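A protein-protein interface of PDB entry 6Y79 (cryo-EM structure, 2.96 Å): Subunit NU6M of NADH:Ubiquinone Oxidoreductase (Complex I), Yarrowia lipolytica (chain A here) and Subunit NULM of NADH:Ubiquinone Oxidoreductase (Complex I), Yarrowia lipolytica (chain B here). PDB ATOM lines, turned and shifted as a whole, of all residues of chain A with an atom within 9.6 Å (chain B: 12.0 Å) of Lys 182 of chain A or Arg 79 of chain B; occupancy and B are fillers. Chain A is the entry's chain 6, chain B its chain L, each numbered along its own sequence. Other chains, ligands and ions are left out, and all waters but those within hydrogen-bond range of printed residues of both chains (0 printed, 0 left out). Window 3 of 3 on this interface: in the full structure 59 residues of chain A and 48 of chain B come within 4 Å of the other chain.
The backbone NH of Asp 79 of chain A sits at hydrogen-bond distance from the side-chain hydroxyl of Tyr 78 of chain B.
The backbone NH of Ile 84 of chain B is in hydrogen-bond range of the backbone carbonyl oxygen of Asp 79 of chain A, at 3.3 Å.
The backbone carbonyl oxygen of Leu 73 of chain B is in hydrogen-bond range of the side-chain hydroxyl of Ser 76 of chain B, at 2.9 Å.
The side-chain hydroxyl of Tyr 78 of chain B sits at hydrogen-bond distance from the backbone carbonyl oxygen of Gly 82 of chain B (3.3 Å).
O of Pro 176 of chain A is in hydrogen-bond range of OG1 of Thr 180 of chain A (2.7 Å).
O of Ile 69 of chain B sits at hydrogen-bond distance from OG of Ser 72 of chain B (2.5 Å).
Among the printed residues, pairs that only touch across the chains: Lys 182 of chain A with Arg 79 of chain B, Ile 179 of chain A with Ser 76 of chain B, Leu 78 of chain A with Tyr 78 of chain B, Leu 78 of chain A with Leu 74 of chain B, Pro 176 of chain A with Ile 69 of chain B, Pro 176 of chain A with Ser 72 of chain B, Ile 179 of chain A with Ser 72 of chain B and Ile 179 of chain A with Leu 73 of chain B.
Of the printed residues of chain B, Asp 79 of chain A touches Tyr 78 and Ile 84.
Of the printed residues of chain B, Ile 179 of chain A touches Ser 72 (3.9 Å), Leu 73 (3.9 Å) and Ser 76 (3.5 Å).
No residue of chain B comes within 4 Å of Thr 180 of chain A.
No residue of chain B comes within 4 Å of Met 181 of chain A.
No residue of chain B comes within 4 Å of His 183 of chain A.
Of chain A, only Lys 182 (3.4 Å) comes within 4 Å of Arg 79 of chain B.
No residue of chain A comes within 4 Å of Leu 80 of chain B.
Of the printed residues of chain A, Ile 84 of chain B touches Asp 79.
The nearest residue of chain B that does not touch Lys 182 of chain A is Leu 80 of chain B (6.0 Å).
The nearest residue of chain A that does not touch Arg 79 of chain B is Thr 180 of chain A (4.2 Å).
Of the 11 printed residues of chain A, 5 touch a printed residue of chain B.
Hydrophobic or aromatic side chains of chain A that line the printed part of chain B: Leu 78, Pro 176 and Ile 179.
Among the printed residues, 10 pairs touch across the chains.
Among the printed residues, no Asp or Glu carboxylate lies within 4 Å of a Lys or Arg side-chain nitrogen of the other chain.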
ATOM      1  N   LEU A  78       0.442  19.203 -28.420  1.00  0.00           N
ATOM      2  CA  LEU A  78       0.553  18.097 -29.361  1.00  0.00           C
ATOM      3  C   LEU A  78       0.394  18.630 -30.778  1.00  0.00           C
ATOM      4  O   LEU A  78      -0.261  19.647 -31.006  1.00  0.00           O
ATOM      5  CB  LEU A  78      -0.483  16.999 -29.094  1.00  0.00           C
ATOM      6  CG  LEU A  78      -0.172  15.993 -27.983  1.00  0.00           C
ATOM      7  CD1 LEU A  78      -0.621  16.480 -26.659  1.00  0.00           C
ATOM      8  CD2 LEU A  78      -0.847  14.710 -28.250  1.00  0.00           C
ATOM      9  N   ASP A  79       0.996  17.932 -31.740  1.00  0.00           N
ATOM     10  CA  ASP A  79       0.984  18.379 -33.127  1.00  0.00           C
ATOM     11  C   ASP A  79      -0.055  17.605 -33.921  1.00  0.00           C
ATOM     12  O   ASP A  79      -0.024  16.372 -33.969  1.00  0.00           O
ATOM     13  CB  ASP A  79       2.353  18.238 -33.785  1.00  0.00           C
ATOM     14  CG  ASP A  79       2.447  19.035 -35.073  1.00  0.00           C
ATOM     15  OD1 ASP A  79       1.961  20.186 -35.095  1.00  0.00           O
ATOM     16  OD2 ASP A  79       2.987  18.511 -36.068  1.00  0.00           O
ATOM     17  N   PRO A 176      -5.362   5.957 -17.539  1.00  0.00           N
ATOM     18  CA  PRO A 176      -4.414   6.971 -18.032  1.00  0.00           C
ATOM     19  C   PRO A 176      -3.063   6.957 -17.348  1.00  0.00           C
ATOM     20  O   PRO A 176      -2.056   7.289 -17.980  1.00  0.00           O
ATOM     21  CB  PRO A 176      -5.159   8.276 -17.759  1.00  0.00           C
ATOM     22  CG  PRO A 176      -6.567   7.916 -17.889  1.00  0.00           C
ATOM     23  CD  PRO A 176      -6.695   6.541 -17.335  1.00  0.00           C
ATOM     24  N   ILE A 177      -3.018   6.604 -16.066  1.00  0.00           N
ATOM     25  CA  ILE A 177      -1.745   6.419 -15.374  1.00  0.00           C
ATOM     26  C   ILE A 177      -1.005   5.225 -15.953  1.00  0.00           C
ATOM     27  O   ILE A 177       0.180   5.308 -16.293  1.00  0.00           O
ATOM     28  CB  ILE A 177      -1.972   6.230 -13.868  1.00  0.00           C
ATOM     29  CG1 ILE A 177      -2.467   7.512 -13.220  1.00  0.00           C
ATOM     30  CG2 ILE A 177      -0.708   5.761 -13.197  1.00  0.00           C
ATOM     31  CD1 ILE A 177      -2.888   7.289 -11.804  1.00  0.00           C
ATOM     32  N   SER A 178      -1.709   4.093 -16.050  1.00  0.00           N
ATOM     33  CA  SER A 178      -1.126   2.830 -16.490  1.00  0.00           C
ATOM     34  C   SER A 178      -0.560   2.915 -17.890  1.00  0.00           C
ATOM     35  O   SER A 178       0.422   2.238 -18.204  1.00  0.00           O
ATOM     36  CB  SER A 178      -2.179   1.743 -16.462  1.00  0.00           C
ATOM     37  OG  SER A 178      -3.141   1.971 -17.465  1.00  0.00           O
ATOM     38  N   ILE A 179      -1.173   3.721 -18.745  1.00  0.00           N
ATOM     39  CA  ILE A 179      -0.619   3.946 -20.071  1.00  0.00           C
ATOM     40  C   ILE A 179       0.692   4.727 -19.987  1.00  0.00           C
ATOM     41  O   ILE A 179       1.737   4.269 -20.457  1.00  0.00           O
ATOM     42  CB  ILE A 179      -1.635   4.675 -20.958  1.00  0.00           C
ATOM     43  CG1 ILE A 179      -2.794   3.763 -21.337  1.00  0.00           C
ATOM     44  CG2 ILE A 179      -0.969   5.102 -22.170  1.00  0.00           C
ATOM     45  CD1 ILE A 179      -3.826   4.468 -22.171  1.00  0.00           C
ATOM     46  N   THR A 180       0.656   5.917 -19.374  1.00  0.00           N
ATOM     47  CA  THR A 180       1.632   6.971 -19.639  1.00  0.00           C
ATOM     48  C   THR A 180       2.758   7.048 -18.623  1.00  0.00           C
ATOM     49  O   THR A 180       3.318   8.133 -18.436  1.00  0.00           O
ATOM     50  CB  THR A 180       0.935   8.333 -19.694  1.00  0.00           C
ATOM     51  OG1 THR A 180       0.322   8.585 -18.424  1.00  0.00           O
ATOM     52  CG2 THR A 180      -0.105   8.382 -20.769  1.00  0.00           C
ATOM     53  N   MET A 181       3.108   5.968 -17.938  1.00  0.00           N
ATOM     54  CA  MET A 181       4.098   6.147 -16.885  1.00  0.00           C
ATOM     55  C   MET A 181       5.500   5.759 -17.335  1.00  0.00           C
ATOM     56  O   MET A 181       6.466   6.495 -17.084  1.00  0.00           O
ATOM     57  CB  MET A 181       3.700   5.374 -15.631  1.00  0.00           C
ATOM     58  CG  MET A 181       4.617   5.779 -14.514  1.00  0.00           C
ATOM     59  SD  MET A 181       4.254   5.437 -12.805  1.00  0.00           S
ATOM     60  CE  MET A 181       5.891   5.783 -12.160  1.00  0.00           C
ATOM     61  N   LYS A 182       5.607   4.625 -18.028  1.00  0.00           N
ATOM     62  CA  LYS A 182       6.857   3.909 -18.277  1.00  0.00           C
ATOM     63  C   LYS A 182       7.596   3.673 -16.957  1.00  0.00           C
ATOM     64  O   LYS A 182       8.556   4.364 -16.607  1.00  0.00           O
ATOM     65  CB  LYS A 182       7.769   4.619 -19.279  1.00  0.00           C
ATOM     66  CG  LYS A 182       7.167   4.798 -20.650  1.00  0.00           C
ATOM     67  CD  LYS A 182       7.092   3.498 -21.413  1.00  0.00           C
ATOM     68  CE  LYS A 182       6.533   3.723 -22.801  1.00  0.00           C
ATOM     69  NZ  LYS A 182       6.467   2.454 -23.558  1.00  0.00           N
ATOM     70  N   HIS A 183       7.038   2.743 -16.182  1.00  0.00           N
ATOM     71  CA  HIS A 183       7.604   2.276 -14.916  1.00  0.00           C
ATOM     72  C   HIS A 183       9.073   1.905 -15.054  1.00  0.00           C
ATOM     73  O   HIS A 183       9.417   0.957 -15.768  1.00  0.00           O
ATOM     74  CB  HIS A 183       6.816   1.060 -14.443  1.00  0.00           C
ATOM     75  CG  HIS A 183       5.387   1.341 -14.119  1.00  0.00           C
ATOM     76  ND1 HIS A 183       4.988   1.927 -12.937  1.00  0.00           N
ATOM     77  CD2 HIS A 183       4.257   1.091 -14.817  1.00  0.00           C
ATOM     78  CE1 HIS A 183       3.672   2.038 -12.928  1.00  0.00           C
ATOM     79  NE2 HIS A 183       3.204   1.538 -14.057  1.00  0.00           N
ATOM     80  N   LYS A 184       9.907   2.642 -14.319  1.00  0.00           N
ATOM     81  CA  LYS A 184      11.382   2.660 -14.363  1.00  0.00           C
ATOM     82  C   LYS A 184      12.059   2.343 -15.706  1.00  0.00           C
ATOM     83  O   LYS A 184      11.597   2.767 -16.767  1.00  0.00           O
ATOM     84  CB  LYS A 184      11.959   1.721 -13.298  1.00  0.00           C
ATOM     85  CG  LYS A 184      11.759   0.243 -13.503  1.00  0.00           C
ATOM     86  CD  LYS A 184      12.582  -0.469 -12.450  1.00  0.00           C
ATOM     87  CE  LYS A 184      12.531  -1.954 -12.596  1.00  0.00           C
ATOM     88  NZ  LYS A 184      11.147  -2.447 -12.303  1.00  0.00           N
ATOM     89  N   ILE B  22      -8.173  14.794 -36.339  1.00  0.00           N
ATOM     90  CA  ILE B  22      -8.668  13.806 -35.402  1.00  0.00           C
ATOM     91  C   ILE B  22      -9.488  14.427 -34.277  1.00  0.00           C
ATOM     92  O   ILE B  22     -10.408  13.777 -33.772  1.00  0.00           O
ATOM     93  CB  ILE B  22      -7.499  12.957 -34.841  1.00  0.00           C
ATOM     94  CG1 ILE B  22      -8.000  11.700 -34.141  1.00  0.00           C
ATOM     95  CG2 ILE B  22      -6.611  13.745 -33.893  1.00  0.00           C
ATOM     96  CD1 ILE B  22      -8.769  10.807 -35.037  1.00  0.00           C
ATOM     97  N   ILE B  69     -10.193   8.914 -20.693  1.00  0.00           N
ATOM     98  CA  ILE B  69      -9.628   7.659 -21.201  1.00  0.00           C
ATOM     99  C   ILE B  69      -9.128   7.834 -22.628  1.00  0.00           C
ATOM    100  O   ILE B  69      -7.968   7.545 -22.939  1.00  0.00           O
ATOM    101  CB  ILE B  69     -10.668   6.524 -21.126  1.00  0.00           C
ATOM    102  CG1 ILE B  69     -10.987   6.119 -19.691  1.00  0.00           C
ATOM    103  CG2 ILE B  69     -10.190   5.305 -21.890  1.00  0.00           C
ATOM    104  CD1 ILE B  69      -9.840   5.606 -18.924  1.00  0.00           C
ATOM    105  N   GLY B  70      -9.989   8.340 -23.509  1.00  0.00           N
ATOM    106  CA  GLY B  70      -9.649   8.459 -24.911  1.00  0.00           C
ATOM    107  C   GLY B  70      -8.599   9.494 -25.218  1.00  0.00           C
ATOM    108  O   GLY B  70      -7.851   9.332 -26.187  1.00  0.00           O
ATOM    109  N   LEU B  71      -8.481  10.531 -24.398  1.00  0.00           N
ATOM    110  CA  LEU B  71      -7.426  11.487 -24.679  1.00  0.00           C
ATOM    111  C   LEU B  71      -6.081  10.978 -24.186  1.00  0.00           C
ATOM    112  O   LEU B  71      -5.055  11.261 -24.816  1.00  0.00           O
ATOM    113  CB  LEU B  71      -7.774  12.852 -24.088  1.00  0.00           C
ATOM    114  CG  LEU B  71      -8.509  13.810 -25.042  1.00  0.00           C
ATOM    115  CD1 LEU B  71      -7.692  14.087 -26.269  1.00  0.00           C
ATOM    116  CD2 LEU B  71      -9.837  13.290 -25.503  1.00  0.00           C
ATOM    117  N   SER B  72      -6.060  10.168 -23.120  1.00  0.00           N
ATOM    118  CA  SER B  72      -4.827   9.442 -22.811  1.00  0.00           C
ATOM    119  C   SER B  72      -4.482   8.418 -23.895  1.00  0.00           C
ATOM    120  O   SER B  72      -3.297   8.176 -24.170  1.00  0.00           O
ATOM    121  CB  SER B  72      -4.945   8.763 -21.450  1.00  0.00           C
ATOM    122  OG  SER B  72      -5.912   7.736 -21.472  1.00  0.00           O
ATOM    123  N   LEU B  73      -5.501   7.826 -24.526  1.00  0.00           N
ATOM    124  CA  LEU B  73      -5.271   6.937 -25.666  1.00  0.00           C
ATOM    125  C   LEU B  73      -4.636   7.676 -26.842  1.00  0.00           C
ATOM    126  O   LEU B  73      -3.742   7.137 -27.506  1.00  0.00           O
ATOM    127  CB  LEU B  73      -6.583   6.281 -26.101  1.00  0.00           C
ATOM    128  CG  LEU B  73      -6.938   4.835 -25.760  1.00  0.00           C
ATOM    129  CD1 LEU B  73      -7.145   4.636 -24.297  1.00  0.00           C
ATOM    130  CD2 LEU B  73      -8.193   4.488 -26.490  1.00  0.00           C
ATOM    131  N   LEU B  74      -5.073   8.915 -27.105  1.00  0.00           N
ATOM    132  CA  LEU B  74      -4.442   9.727 -28.150  1.00  0.00           C
ATOM    133  C   LEU B  74      -3.009  10.093 -27.791  1.00  0.00           C
ATOM    134  O   LEU B  74      -2.149  10.162 -28.675  1.00  0.00           O
ATOM    135  CB  LEU B  74      -5.247  10.997 -28.430  1.00  0.00           C
ATOM    136  CG  LEU B  74      -4.784  11.915 -29.574  1.00  0.00           C
ATOM    137  CD1 LEU B  74      -5.924  12.491 -30.294  1.00  0.00           C
ATOM    138  CD2 LEU B  74      -3.997  13.105 -29.104  1.00  0.00           C
ATOM    139  N   VAL B  75      -2.740  10.365 -26.513  1.00  0.00           N
ATOM    140  CA  VAL B  75      -1.377  10.703 -26.105  1.00  0.00           C
ATOM    141  C   VAL B  75      -0.441   9.520 -26.330  1.00  0.00           C
ATOM    142  O   VAL B  75       0.672   9.684 -26.844  1.00  0.00           O
ATOM    143  CB  VAL B  75      -1.362  11.192 -24.644  1.00  0.00           C
ATOM    144  CG1 VAL B  75       0.052  11.310 -24.113  1.00  0.00           C
ATOM    145  CG2 VAL B  75      -2.044  12.531 -24.540  1.00  0.00           C
ATOM    146  N   SER B  76      -0.902   8.303 -26.027  1.00  0.00           N
ATOM    147  CA  SER B  76      -0.076   7.126 -26.299  1.00  0.00           C
ATOM    148  C   SER B  76       0.027   6.820 -27.785  1.00  0.00           C
ATOM    149  O   SER B  76       0.994   6.188 -28.221  1.00  0.00           O
ATOM    150  CB  SER B  76      -0.609   5.905 -25.583  1.00  0.00           C
ATOM    151  OG  SER B  76      -1.857   5.493 -26.095  1.00  0.00           O
ATOM    152  N   TYR B  77      -0.988   7.199 -28.569  1.00  0.00           N
ATOM    153  CA  TYR B  77      -0.852   7.139 -30.021  1.00  0.00           C
ATOM    154  C   TYR B  77       0.252   8.066 -30.496  1.00  0.00           C
ATOM    155  O   TYR B  77       0.995   7.731 -31.421  1.00  0.00           O
ATOM    156  CB  TYR B  77      -2.176   7.507 -30.685  1.00  0.00           C
ATOM    157  CG  TYR B  77      -2.173   7.444 -32.197  1.00  0.00           C
ATOM    158  CD1 TYR B  77      -2.437   6.260 -32.855  1.00  0.00           C
ATOM    159  CD2 TYR B  77      -1.934   8.580 -32.968  1.00  0.00           C
ATOM    160  CE1 TYR B  77      -2.442   6.196 -34.230  1.00  0.00           C
ATOM    161  CE2 TYR B  77      -1.928   8.521 -34.340  1.00  0.00           C
ATOM    162  CZ  TYR B  77      -2.184   7.327 -34.964  1.00  0.00           C
ATOM    163  OH  TYR B  77      -2.183   7.262 -36.334  1.00  0.00           O
ATOM    164  N   TYR B  78       0.374   9.224 -29.861  1.00  0.00           N
ATOM    165  CA  TYR B  78       1.332  10.254 -30.228  1.00  0.00           C
ATOM    166  C   TYR B  78       2.742   9.988 -29.713  1.00  0.00           C
ATOM    167  O   TYR B  78       3.684  10.589 -30.231  1.00  0.00           O
ATOM    168  CB  TYR B  78       0.817  11.597 -29.700  1.00  0.00           C
ATOM    169  CG  TYR B  78       1.633  12.810 -30.052  1.00  0.00           C
ATOM    170  CD1 TYR B  78       1.470  13.445 -31.269  1.00  0.00           C
ATOM    171  CD2 TYR B  78       2.553  13.332 -29.152  1.00  0.00           C
ATOM    172  CE1 TYR B  78       2.211  14.554 -31.587  1.00  0.00           C
ATOM    173  CE2 TYR B  78       3.301  14.433 -29.467  1.00  0.00           C
ATOM    174  CZ  TYR B  78       3.123  15.041 -30.681  1.00  0.00           C
ATOM    175  OH  TYR B  78       3.866  16.149 -30.989  1.00  0.00           O
ATOM    176  N   ARG B  79       2.907   9.116 -28.707  1.00  0.00           N
ATOM    177  CA  ARG B  79       4.227   8.855 -28.124  1.00  0.00           C
ATOM    178  C   ARG B  79       5.227   8.334 -29.144  1.00  0.00           C
ATOM    179  O   ARG B  79       6.375   8.787 -29.186  1.00  0.00           O
ATOM    180  CB  ARG B  79       4.138   7.828 -27.001  1.00  0.00           C
ATOM    181  CG  ARG B  79       3.380   8.221 -25.782  1.00  0.00           C
ATOM    182  CD  ARG B  79       3.476   7.113 -24.761  1.00  0.00           C
ATOM    183  NE  ARG B  79       4.861   6.926 -24.368  1.00  0.00           N
ATOM    184  CZ  ARG B  79       5.378   7.412 -23.249  1.00  0.00           C
ATOM    185  NH1 ARG B  79       6.653   7.212 -22.968  1.00  0.00           N
ATOM    186  NH2 ARG B  79       4.614   8.094 -22.410  1.00  0.00           N
ATOM    187  N   LEU B  80       4.816   7.376 -29.961  1.00  0.00           N
ATOM    188  CA  LEU B  80       5.721   6.731 -30.894  1.00  0.00           C
ATOM    189  C   LEU B  80       5.748   7.409 -32.248  1.00  0.00           C
ATOM    190  O   LEU B  80       6.703   7.225 -33.005  1.00  0.00           O
ATOM    191  CB  LEU B  80       5.312   5.278 -31.083  1.00  0.00           C
ATOM    192  CG  LEU B  80       5.235   4.375 -29.866  1.00  0.00           C
ATOM    193  CD1 LEU B  80       4.584   3.123 -30.316  1.00  0.00           C
ATOM    194  CD2 LEU B  80       6.613   4.086 -29.327  1.00  0.00           C
ATOM    195  N   ARG B  81       4.717   8.172 -32.567  1.00  0.00           N
ATOM    196  CA  ARG B  81       4.636   8.935 -33.801  1.00  0.00           C
ATOM    197  C   ARG B  81       4.448  10.380 -33.391  1.00  0.00           C
ATOM    198  O   ARG B  81       3.338  10.773 -33.027  1.00  0.00           O
ATOM    199  CB  ARG B  81       3.464   8.469 -34.663  1.00  0.00           C
ATOM    200  CG  ARG B  81       3.746   7.259 -35.515  1.00  0.00           C
ATOM    201  CD  ARG B  81       3.517   5.971 -34.753  1.00  0.00           C
ATOM    202  NE  ARG B  81       2.100   5.722 -34.523  1.00  0.00           N
ATOM    203  CZ  ARG B  81       1.630   4.953 -33.551  1.00  0.00           C
ATOM    204  NH1 ARG B  81       2.449   4.368 -32.696  1.00  0.00           N
ATOM    205  NH2 ARG B  81       0.339   4.777 -33.424  1.00  0.00           N
ATOM    206  N   GLY B  82       5.486  11.203 -33.520  1.00  0.00           N
ATOM    207  CA  GLY B  82       5.414  12.579 -33.049  1.00  0.00           C
ATOM    208  C   GLY B  82       4.588  13.531 -33.896  1.00  0.00           C
ATOM    209  O   GLY B  82       4.772  14.751 -33.858  1.00  0.00           O
ATOM    210  N   VAL B  83       3.657  12.963 -34.650  1.00  0.00           N
ATOM    211  CA  VAL B  83       2.818  13.646 -35.610  1.00  0.00           C
ATOM    212  C   VAL B  83       1.472  12.947 -35.546  1.00  0.00           C
ATOM    213  O   VAL B  83       1.384  11.767 -35.201  1.00  0.00           O
ATOM    214  CB  VAL B  83       3.463  13.594 -37.022  1.00  0.00           C
ATOM    215  CG1 VAL B  83       3.606  12.156 -37.528  1.00  0.00           C
ATOM    216  CG2 VAL B  83       2.712  14.438 -38.029  1.00  0.00           C
ATOM    217  N   ILE B  84       0.409  13.696 -35.789  1.00  0.00           N
ATOM    218  CA  ILE B  84      -0.901  13.115 -36.022  1.00  0.00           C
ATOM    219  C   ILE B  84      -1.325  13.513 -37.421  1.00  0.00           C
ATOM    220  O   ILE B  84      -1.317  14.699 -37.763  1.00  0.00           O
ATOM    221  CB  ILE B  84      -1.920  13.556 -34.964  1.00  0.00           C
ATOM    222  CG1 ILE B  84      -1.489  13.024 -33.602  1.00  0.00           C
ATOM    223  CG2 ILE B  84      -3.279  13.015 -35.303  1.00  0.00           C
ATOM    224  CD1 ILE B  84      -2.358  13.469 -32.487  1.00  0.00           C
ATOM    225  N   ASN B  85      -1.647  12.517 -38.236  1.00  0.00           N
ATOM    226  CA  ASN B  85      -1.956  12.741 -39.633  1.00  0.00           C
ATOM    227  C   ASN B  85      -3.271  13.490 -39.787  1.00  0.00           C
ATOM    228  O   ASN B  85      -4.151  13.456 -38.923  1.00  0.00           O
ATOM    229  CB  ASN B  85      -2.030  11.415 -40.376  1.00  0.00           C
ATOM    230  CG  ASN B  85      -0.705  10.698 -40.411  1.00  0.00           C
ATOM    231  OD1 ASN B  85       0.344  11.316 -40.584  1.00  0.00           O
ATOM    232  ND2 ASN B  85      -0.743   9.381 -40.248  1.00  0.00           N
ATOM    233  N   ILE B  89      -6.063   8.264 -38.344  1.00  0.00           N
ATOM    234  CA  ILE B  89      -5.186   7.279 -37.734  1.00  0.00           C
ATOM    235  C   ILE B  89      -4.797   6.212 -38.747  1.00  0.00           C
ATOM    236  O   ILE B  89      -3.876   5.430 -38.514  1.00  0.00           O
ATOM    237  CB  ILE B  89      -5.844   6.643 -36.506  1.00  0.00           C
ATOM    238  CG1 ILE B  89      -7.124   5.922 -36.914  1.00  0.00           C
ATOM    239  CG2 ILE B  89      -6.136   7.693 -35.449  1.00  0.00           C
ATOM    240  CD1 ILE B  89      -7.729   5.118 -35.818  1.00  0.00           C
